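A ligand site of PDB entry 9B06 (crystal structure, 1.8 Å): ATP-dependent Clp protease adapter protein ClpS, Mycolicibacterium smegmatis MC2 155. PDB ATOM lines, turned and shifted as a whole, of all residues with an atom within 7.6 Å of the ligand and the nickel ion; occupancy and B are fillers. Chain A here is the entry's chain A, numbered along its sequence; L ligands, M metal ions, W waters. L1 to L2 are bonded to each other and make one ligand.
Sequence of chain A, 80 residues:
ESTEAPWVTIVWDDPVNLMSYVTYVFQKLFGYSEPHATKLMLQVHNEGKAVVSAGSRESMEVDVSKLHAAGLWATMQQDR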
ATOM      1  N   VAL A  11     -13.842 -28.489  29.274  1.00  0.00           N
ATOM      2  CA  VAL A  11     -13.430 -27.856  28.024  1.00  0.00           C
ATOM      3  C   VAL A  11     -14.425 -26.754  27.707  1.00  0.00           C
ATOM      4  O   VAL A  11     -15.645 -26.972  27.780  1.00  0.00           O
ATOM      5  CB  VAL A  11     -13.289 -28.884  26.875  1.00  0.00           C
ATOM      6  CG1 VAL A  11     -13.118 -28.208  25.516  1.00  0.00           C
ATOM      7  CG2 VAL A  11     -12.101 -29.786  27.155  1.00  0.00           C
ATOM      8  N   TRP A  12     -13.904 -25.587  27.351  1.00  0.00           N
ATOM      9  CA  TRP A  12     -14.692 -24.386  27.080  1.00  0.00           C
ATOM     10  C   TRP A  12     -14.785 -24.148  25.584  1.00  0.00           C
ATOM     11  O   TRP A  12     -13.814 -24.358  24.850  1.00  0.00           O
ATOM     12  CB  TRP A  12     -14.022 -23.187  27.739  1.00  0.00           C
ATOM     13  CG  TRP A  12     -13.974 -23.327  29.231  1.00  0.00           C
ATOM     14  CD1 TRP A  12     -13.017 -23.967  29.960  1.00  0.00           C
ATOM     15  CD2 TRP A  12     -14.933 -22.838  30.175  1.00  0.00           C
ATOM     16  NE1 TRP A  12     -13.318 -23.920  31.300  1.00  0.00           N
ATOM     17  CE2 TRP A  12     -14.493 -23.217  31.461  1.00  0.00           C
ATOM     18  CE3 TRP A  12     -16.118 -22.103  30.054  1.00  0.00           C
ATOM     19  CZ2 TRP A  12     -15.184 -22.887  32.610  1.00  0.00           C
ATOM     20  CZ3 TRP A  12     -16.809 -21.780  31.209  1.00  0.00           C
ATOM     21  CH2 TRP A  12     -16.351 -22.176  32.474  1.00  0.00           C
ATOM     22  N   ASP A  13     -15.946 -23.699  25.146  1.00  0.00           N
ATOM     23  CA  ASP A  13     -16.108 -23.368  23.735  1.00  0.00           C
ATOM     24  C   ASP A  13     -15.174 -22.242  23.312  1.00  0.00           C
ATOM     25  O   ASP A  13     -14.961 -21.293  24.038  1.00  0.00           O
ATOM     26  CB  ASP A  13     -17.562 -22.959  23.488  1.00  0.00           C
ATOM     27  CG  ASP A  13     -17.876 -22.837  22.021  1.00  0.00           C
ATOM     28  OD1 ASP A  13     -17.353 -23.650  21.261  1.00  0.00           O
ATOM     29  OD2 ASP A  13     -18.627 -21.924  21.610  1.00  0.00           O
ATOM     30  N   ASP A  14     -14.588 -22.376  22.106  1.00  0.00           N
ATOM     31  CA  ASP A  14     -13.689 -21.380  21.550  1.00  0.00           C
ATOM     32  C   ASP A  14     -14.074 -21.132  20.096  1.00  0.00           C
ATOM     33  O   ASP A  14     -14.638 -22.029  19.450  1.00  0.00           O
ATOM     34  CB  ASP A  14     -12.215 -21.811  21.654  1.00  0.00           C
ATOM     35  CG  ASP A  14     -11.798 -22.820  20.628  1.00  0.00           C
ATOM     36  OD1 ASP A  14     -11.454 -22.384  19.499  1.00  0.00           O
ATOM     37  OD2 ASP A  14     -11.752 -24.037  20.955  1.00  0.00           O
ATOM     38  N   PRO A  15     -13.818 -19.940  19.559  1.00  0.00           N
ATOM     39  CA  PRO A  15     -14.350 -19.604  18.234  1.00  0.00           C
ATOM     40  C   PRO A  15     -13.508 -20.051  17.052  1.00  0.00           C
ATOM     41  O   PRO A  15     -13.858 -19.692  15.919  1.00  0.00           O
ATOM     42  CB  PRO A  15     -14.402 -18.078  18.301  1.00  0.00           C
ATOM     43  CG  PRO A  15     -13.226 -17.706  19.090  1.00  0.00           C
ATOM     44  CD  PRO A  15     -13.075 -18.790  20.124  1.00  0.00           C
ATOM     45  N   VAL A  16     -12.432 -20.807  17.259  1.00  0.00           N
ATOM     46  CA  VAL A  16     -11.478 -21.167  16.204  1.00  0.00           C
ATOM     47  C   VAL A  16     -11.521 -22.653  15.896  1.00  0.00           C
ATOM     48  O   VAL A  16     -11.604 -23.040  14.736  1.00  0.00           O
ATOM     49  CB  VAL A  16     -10.047 -20.687  16.531  1.00  0.00           C
ATOM     50  CG1 VAL A  16      -9.070 -21.041  15.403  1.00  0.00           C
ATOM     51  CG2 VAL A  16     -10.044 -19.182  16.798  1.00  0.00           C
ATOM     52  N   ASN A  17     -11.396 -23.513  16.922  1.00  0.00           N
ATOM     53  CA  ASN A  17     -11.196 -24.941  16.690  1.00  0.00           C
ATOM     54  C   ASN A  17     -12.372 -25.571  15.976  1.00  0.00           C
ATOM     55  O   ASN A  17     -13.531 -25.228  16.231  1.00  0.00           O
ATOM     56  CB  ASN A  17     -10.971 -25.681  18.016  1.00  0.00           C
ATOM     57  CG  ASN A  17      -9.537 -25.587  18.500  1.00  0.00           C
ATOM     58  OD1 ASN A  17      -8.600 -25.906  17.773  1.00  0.00           O
ATOM     59  ND2 ASN A  17      -9.370 -25.147  19.744  1.00  0.00           N
ATOM     60  N   LEU A  18     -12.070 -26.458  15.040  1.00  0.00           N
ATOM     61  CA  LEU A  18     -13.090 -27.183  14.304  1.00  0.00           C
ATOM     62  C   LEU A  18     -13.828 -28.166  15.219  1.00  0.00           C
ATOM     63  O   LEU A  18     -13.200 -28.850  16.035  1.00  0.00           O
ATOM     64  CB  LEU A  18     -12.437 -27.987  13.183  1.00  0.00           C
ATOM     65  CG  LEU A  18     -11.938 -27.232  11.944  1.00  0.00           C
ATOM     66  CD1 LEU A  18     -10.959 -28.075  11.164  1.00  0.00           C
ATOM     67  CD2 LEU A  18     -13.125 -26.826  11.062  1.00  0.00           C
ATOM     68  N   MET A  19     -15.157 -28.251  15.039  1.00  0.00           N
ATOM     69  CA  MET A  19     -15.945 -29.285  15.710  1.00  0.00           C
ATOM     70  C   MET A  19     -15.347 -30.670  15.469  1.00  0.00           C
ATOM     71  O   MET A  19     -15.190 -31.451  16.403  1.00  0.00           O
ATOM     72  CB  MET A  19     -17.397 -29.254  15.223  1.00  0.00           C
ATOM     73  CG  MET A  19     -18.132 -27.979  15.551  1.00  0.00           C
ATOM     74  SD  MET A  19     -19.789 -27.967  14.828  1.00  0.00           S
ATOM     75  CE  MET A  19     -19.402 -27.704  13.090  1.00  0.00           C
ATOM     76  N   SER A  20     -14.922 -30.947  14.225  1.00  0.00           N
ATOM     77  CA  SER A  20     -14.380 -32.275  13.927  1.00  0.00           C
ATOM     78  C   SER A  20     -13.070 -32.509  14.672  1.00  0.00           C
ATOM     79  O   SER A  20     -12.808 -33.618  15.139  1.00  0.00           O
ATOM     80  CB  SER A  20     -14.170 -32.425  12.423  1.00  0.00           C
ATOM     81  OG  SER A  20     -13.254 -31.438  11.968  1.00  0.00           O
ATOM     82  N   TYR A  21     -12.290 -31.446  14.849  1.00  0.00           N
ATOM     83  CA  TYR A  21     -11.039 -31.559  15.570  1.00  0.00           C
ATOM     84  C   TYR A  21     -11.289 -31.888  17.015  1.00  0.00           C
ATOM     85  O   TYR A  21     -10.607 -32.741  17.583  1.00  0.00           O
ATOM     86  CB  TYR A  21     -10.256 -30.236  15.463  1.00  0.00           C
ATOM     87  CG  TYR A  21      -8.936 -30.303  16.178  1.00  0.00           C
ATOM     88  CD1 TYR A  21      -7.957 -31.199  15.785  1.00  0.00           C
ATOM     89  CD2 TYR A  21      -8.663 -29.450  17.237  1.00  0.00           C
ATOM     90  CE1 TYR A  21      -6.731 -31.245  16.429  1.00  0.00           C
ATOM     91  CE2 TYR A  21      -7.445 -29.500  17.892  1.00  0.00           C
ATOM     92  CZ  TYR A  21      -6.494 -30.391  17.489  1.00  0.00           C
ATOM     93  OH  TYR A  21      -5.271 -30.450  18.116  1.00  0.00           O
ATOM     94  N   VAL A  22     -12.299 -31.245  17.619  1.00  0.00           N
ATOM     95  CA  VAL A  22     -12.558 -31.453  19.040  1.00  0.00           C
ATOM     96  C   VAL A  22     -13.008 -32.869  19.305  1.00  0.00           C
ATOM     97  O   VAL A  22     -12.520 -33.514  20.236  1.00  0.00           O
ATOM     98  CB  VAL A  22     -13.541 -30.409  19.590  1.00  0.00           C
ATOM     99  CG1 VAL A  22     -13.953 -30.741  21.013  1.00  0.00           C
ATOM    100  CG2 VAL A  22     -12.927 -29.001  19.509  1.00  0.00           C
ATOM    101  N   THR A  23     -13.904 -33.408  18.467  1.00  0.00           N
ATOM    102  CA  THR A  23     -14.290 -34.820  18.560  1.00  0.00           C
ATOM    103  C   THR A  23     -13.075 -35.744  18.472  1.00  0.00           C
ATOM    104  O   THR A  23     -12.904 -36.654  19.273  1.00  0.00           O
ATOM    105  CB  THR A  23     -15.289 -35.144  17.460  1.00  0.00           C
ATOM    106  OG1 THR A  23     -16.438 -34.322  17.613  1.00  0.00           O
ATOM    107  CG2 THR A  23     -15.710 -36.601  17.463  1.00  0.00           C
ATOM    108  N   PHE A  26     -10.832 -35.662  21.637  1.00  0.00           N
ATOM    109  CA  PHE A  26     -11.356 -36.404  22.779  1.00  0.00           C
ATOM    110  C   PHE A  26     -11.148 -37.898  22.591  1.00  0.00           C
ATOM    111  O   PHE A  26     -10.880 -38.614  23.560  1.00  0.00           O
ATOM    112  CB  PHE A  26     -12.845 -36.103  23.010  1.00  0.00           C
ATOM    113  CG  PHE A  26     -13.185 -34.677  23.451  1.00  0.00           C
ATOM    114  CD1 PHE A  26     -12.258 -33.829  24.036  1.00  0.00           C
ATOM    115  CD2 PHE A  26     -14.479 -34.203  23.304  1.00  0.00           C
ATOM    116  CE1 PHE A  26     -12.593 -32.567  24.445  1.00  0.00           C
ATOM    117  CE2 PHE A  26     -14.836 -32.939  23.716  1.00  0.00           C
ATOM    118  CZ  PHE A  26     -13.910 -32.122  24.278  1.00  0.00           C
ATOM    119  N   LEU A  40     -19.785 -35.059  23.744  1.00  0.00           N
ATOM    120  CA  LEU A  40     -19.102 -34.063  24.564  1.00  0.00           C
ATOM    121  C   LEU A  40     -18.781 -32.820  23.753  1.00  0.00           C
ATOM    122  O   LEU A  40     -18.895 -31.693  24.266  1.00  0.00           O
ATOM    123  CB  LEU A  40     -17.829 -34.659  25.139  1.00  0.00           C
ATOM    124  CG  LEU A  40     -18.030 -35.752  26.192  1.00  0.00           C
ATOM    125  CD1 LEU A  40     -16.707 -36.452  26.505  1.00  0.00           C
ATOM    126  CD2 LEU A  40     -18.636 -35.189  27.459  1.00  0.00           C
ATOM    127  N   MET A  41     -18.309 -33.002  22.517  1.00  0.00           N
ATOM    128  CA  MET A  41     -18.060 -31.879  21.632  1.00  0.00           C
ATOM    129  C   MET A  41     -19.312 -31.020  21.491  1.00  0.00           C
ATOM    130  O   MET A  41     -19.244 -29.782  21.498  1.00  0.00           O
ATOM    131  CB  MET A  41     -17.564 -32.382  20.279  1.00  0.00           C
ATOM    132  CG  MET A  41     -17.268 -31.272  19.249  1.00  0.00           C
ATOM    133  SD  MET A  41     -18.710 -30.685  18.320  1.00  0.00           S
ATOM    134  CE  MET A  41     -18.972 -32.152  17.290  1.00  0.00           C
ATOM    135  N   LEU A  42     -20.453 -31.651  21.248  1.00  0.00           N
ATOM    136  CA  LEU A  42     -21.657 -30.858  21.005  1.00  0.00           C
ATOM    137  C   LEU A  42     -22.100 -30.138  22.280  1.00  0.00           C
ATOM    138  O   LEU A  42     -22.626 -29.014  22.204  1.00  0.00           O
ATOM    139  CB  LEU A  42     -22.775 -31.760  20.498  1.00  0.00           C
ATOM    140  CG  LEU A  42     -22.542 -32.241  19.057  1.00  0.00           C
ATOM    141  CD1 LEU A  42     -23.478 -33.400  18.724  1.00  0.00           C
ATOM    142  CD2 LEU A  42     -22.732 -31.117  18.074  1.00  0.00           C
ATOM    143  N   GLN A  43     -21.882 -30.778  23.426  1.00  0.00           N
ATOM    144  CA  GLN A  43     -22.183 -30.115  24.693  1.00  0.00           C
ATOM    145  C   GLN A  43     -21.313 -28.884  24.874  1.00  0.00           C
ATOM    146  O   GLN A  43     -21.811 -27.844  25.324  1.00  0.00           O
ATOM    147  CB  GLN A  43     -21.993 -31.086  25.855  1.00  0.00           C
ATOM    148  CG  GLN A  43     -22.512 -30.541  27.180  1.00  0.00           C
ATOM    149  CD  GLN A  43     -22.272 -31.480  28.318  1.00  0.00           C
ATOM    150  OE1 GLN A  43     -21.598 -32.505  28.165  1.00  0.00           O
ATOM    151  NE2 GLN A  43     -22.849 -31.163  29.483  1.00  0.00           N
ATOM    152  N   VAL A  44     -20.004 -28.999  24.571  1.00  0.00           N
ATOM    153  CA  VAL A  44     -19.133 -27.820  24.557  1.00  0.00           C
ATOM    154  C   VAL A  44     -19.722 -26.755  23.659  1.00  0.00           C
ATOM    155  O   VAL A  44     -19.831 -25.582  24.037  1.00  0.00           O
ATOM    156  CB  VAL A  44     -17.709 -28.180  24.087  1.00  0.00           C
ATOM    157  CG1 VAL A  44     -16.888 -26.897  23.881  1.00  0.00           C
ATOM    158  CG2 VAL A  44     -16.993 -29.102  25.070  1.00  0.00           C
ATOM    159  N   HIS A  45     -20.121 -27.144  22.447  1.00  0.00           N
ATOM    160  CA  HIS A  45     -20.497 -26.129  21.486  1.00  0.00           C
ATOM    161  C   HIS A  45     -21.853 -25.533  21.803  1.00  0.00           C
ATOM    162  O   HIS A  45     -22.061 -24.343  21.538  1.00  0.00           O
ATOM    163  CB  HIS A  45     -20.529 -26.730  20.086  1.00  0.00           C
ATOM    164  CG  HIS A  45     -20.374 -25.717  18.996  1.00  0.00           C
ATOM    165  ND1 HIS A  45     -20.836 -25.951  17.723  1.00  0.00           N
ATOM    166  CD2 HIS A  45     -19.775 -24.506  18.957  1.00  0.00           C
ATOM    167  CE1 HIS A  45     -20.529 -24.920  16.948  1.00  0.00           C
ATOM    168  NE2 HIS A  45     -19.882 -24.031  17.681  1.00  0.00           N
ATOM    169  N   ASN A  46     -22.775 -26.309  22.382  1.00  0.00           N
ATOM    170  CA  ASN A  46     -24.147 -25.859  22.593  1.00  0.00           C
ATOM    171  C   ASN A  46     -24.456 -25.358  23.993  1.00  0.00           C
ATOM    172  O   ASN A  46     -25.395 -24.578  24.158  1.00  0.00           O
ATOM    173  CB  ASN A  46     -25.117 -26.971  22.206  1.00  0.00           C
ATOM    174  CG  ASN A  46     -25.197 -27.159  20.701  1.00  0.00           C
ATOM    175  OD1 ASN A  46     -25.323 -26.185  19.949  1.00  0.00           O
ATOM    176  ND2 ASN A  46     -25.098 -28.381  20.260  1.00  0.00           N
ATOM    177  N   LEU A  72      -6.932 -26.781  22.939  1.00  0.00           N
ATOM    178  CA  LEU A  72      -8.280 -26.620  23.463  1.00  0.00           C
ATOM    179  C   LEU A  72      -8.267 -25.845  24.777  1.00  0.00           C
ATOM    180  O   LEU A  72      -7.298 -25.891  25.534  1.00  0.00           O
ATOM    181  CB  LEU A  72      -8.916 -27.997  23.697  1.00  0.00           C
ATOM    182  CG  LEU A  72      -9.653 -28.596  22.491  1.00  0.00           C
ATOM    183  CD1 LEU A  72      -8.771 -28.765  21.290  1.00  0.00           C
ATOM    184  CD2 LEU A  72     -10.336 -29.891  22.861  1.00  0.00           C
HETATM  185  N1  LIG L   1     -16.929 -23.175  18.318  1.00  0.00           N
HETATM  186  C1  LIG L   1     -16.279 -24.097  17.370  1.00  0.00           C
HETATM  187  C2  LIG L   1     -16.768 -23.833  15.937  1.00  0.00           C
HETATM  188  C3  LIG L   1     -16.494 -25.569  17.744  1.00  0.00           C
HETATM  189  C4  LIG L   1     -16.200 -25.985  19.193  1.00  0.00           C
HETATM  190  C5  LIG L   1     -16.468 -27.439  19.460  1.00  0.00           C
HETATM  191  C6  LIG L   1     -14.778 -25.581  19.651  1.00  0.00           C
HETATM  192  O1  LIG L   1     -17.818 -23.237  15.752  1.00  0.00           O
HETATM  193  N1  LG2 L   2     -15.995 -24.259  14.943  1.00  0.00           N
HETATM  194  C1  LG2 L   2     -16.275 -23.951  13.518  1.00  0.00           C
HETATM  195  C2  LG2 L   2     -16.505 -25.194  12.692  1.00  0.00           C
HETATM  196  O1  LG2 L   2     -17.027 -25.091  11.588  1.00  0.00           O
HETATM  197  C3  LG2 L   2     -15.102 -23.181  12.885  1.00  0.00           C
HETATM  198  O2  LG2 L   2     -13.877 -23.896  13.080  1.00  0.00           O
HETATM  199  C4  LG2 L   2     -14.986 -21.804  13.493  1.00  0.00           C
HETATM  200  O3  LG2 L   2     -16.159 -26.295  13.105  1.00  0.00           O
HETATM  201 NI    NI M   1     -18.687 -22.426  17.335  1.00  0.00          NI
HETATM  202  O   HOH W   1     -19.272 -24.094  11.440  1.00  0.00           O
HETATM  203  O   HOH W   2     -12.343 -23.146  10.607  1.00  0.00           O
HETATM  204  O   HOH W   3     -16.722 -26.732   9.479  1.00  0.00           O
HETATM  205  O   HOH W   4     -20.403 -21.618  16.250  1.00  0.00           O
HETATM  206  O   HOH W   5     -19.450 -21.457  19.088  1.00  0.00           O
HETATM  207  O   HOH W   6     -17.793 -20.620  16.889  1.00  0.00           O
HETATM  208  O   HOH W   7     -16.160 -19.193  15.005  1.00  0.00           O
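The backbone carbonyl oxygen (O) of Asp 14 sits close to a nitrogen (N1) of LIG L1 (2.8 Å).
N of Met 19 is in hydrogen-bond range of O3 of LG2 L2, at 2.9 Å.
An oxygen (O2) of LG2 L2 sits at hydrogen-bond distance from the backbone carbonyl oxygen (O) of Val 16 (2.9 Å).
A nitrogen (N1) of LG2 L2 sits at hydrogen-bond distance from the backbone carbonyl oxygen of Asn 17, at 2.9 Å.
The side-chain carboxylate of Asp 13 sits close to a nitrogen (N1) of LIG L1.
A ring nitrogen (ND1) of His 45 is in hydrogen-bond range of the side-chain sulfur of Met 19 (3.7 Å).
The side-chain carboxylate (OD1) of Asp 14 sits at hydrogen-bond distance from the backbone NH (N) of Val 16 (2.9 Å).
OD1 of Asp 14 lies within hydrogen-bond range of N of Asn 17, 2.8 Å away.
The backbone carbonyl oxygen (O) of Met 19 is in hydrogen-bond range of the side-chain hydroxyl (OG1) of Thr 23 (3.4 Å).
Pro 15 touches the ligand.
Leu 18 touches the ligand.
CG2 of Val 22 touches C5 of LIG L1 (3.9 Å).
CG of Met 41 touches C5 of LIG L1 (3.9 Å).
Hydrophobic or aromatic side chains within 4 Å of the ligand: Leu 18, Met 19, Val 22, Met 41 and His 45.
Within 4 Å of the ligand: Asp 13, Asp 14, Pro 15, Val 16, Asn 17, Leu 18, Met 19, Val 22, Met 41 and His 45.
The nearest printed residue that does not touch the ligand is Val 44 (4.5 Å).
One residue has an atom within 4 Å of the nickel ion: His 45.
The nickel ion is bound by an oxygen (O1) of LIG L1 (2.0 Å), a ring nitrogen (NE2) of His 45 (2.0 Å), water W6 (2.1 Å), water W5 (2.1 Å), a nitrogen (N1) of LIG L1 (2.1 Å) and water W4 (2.2 Å).
The nickel ion has six donor atoms within binding distance.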
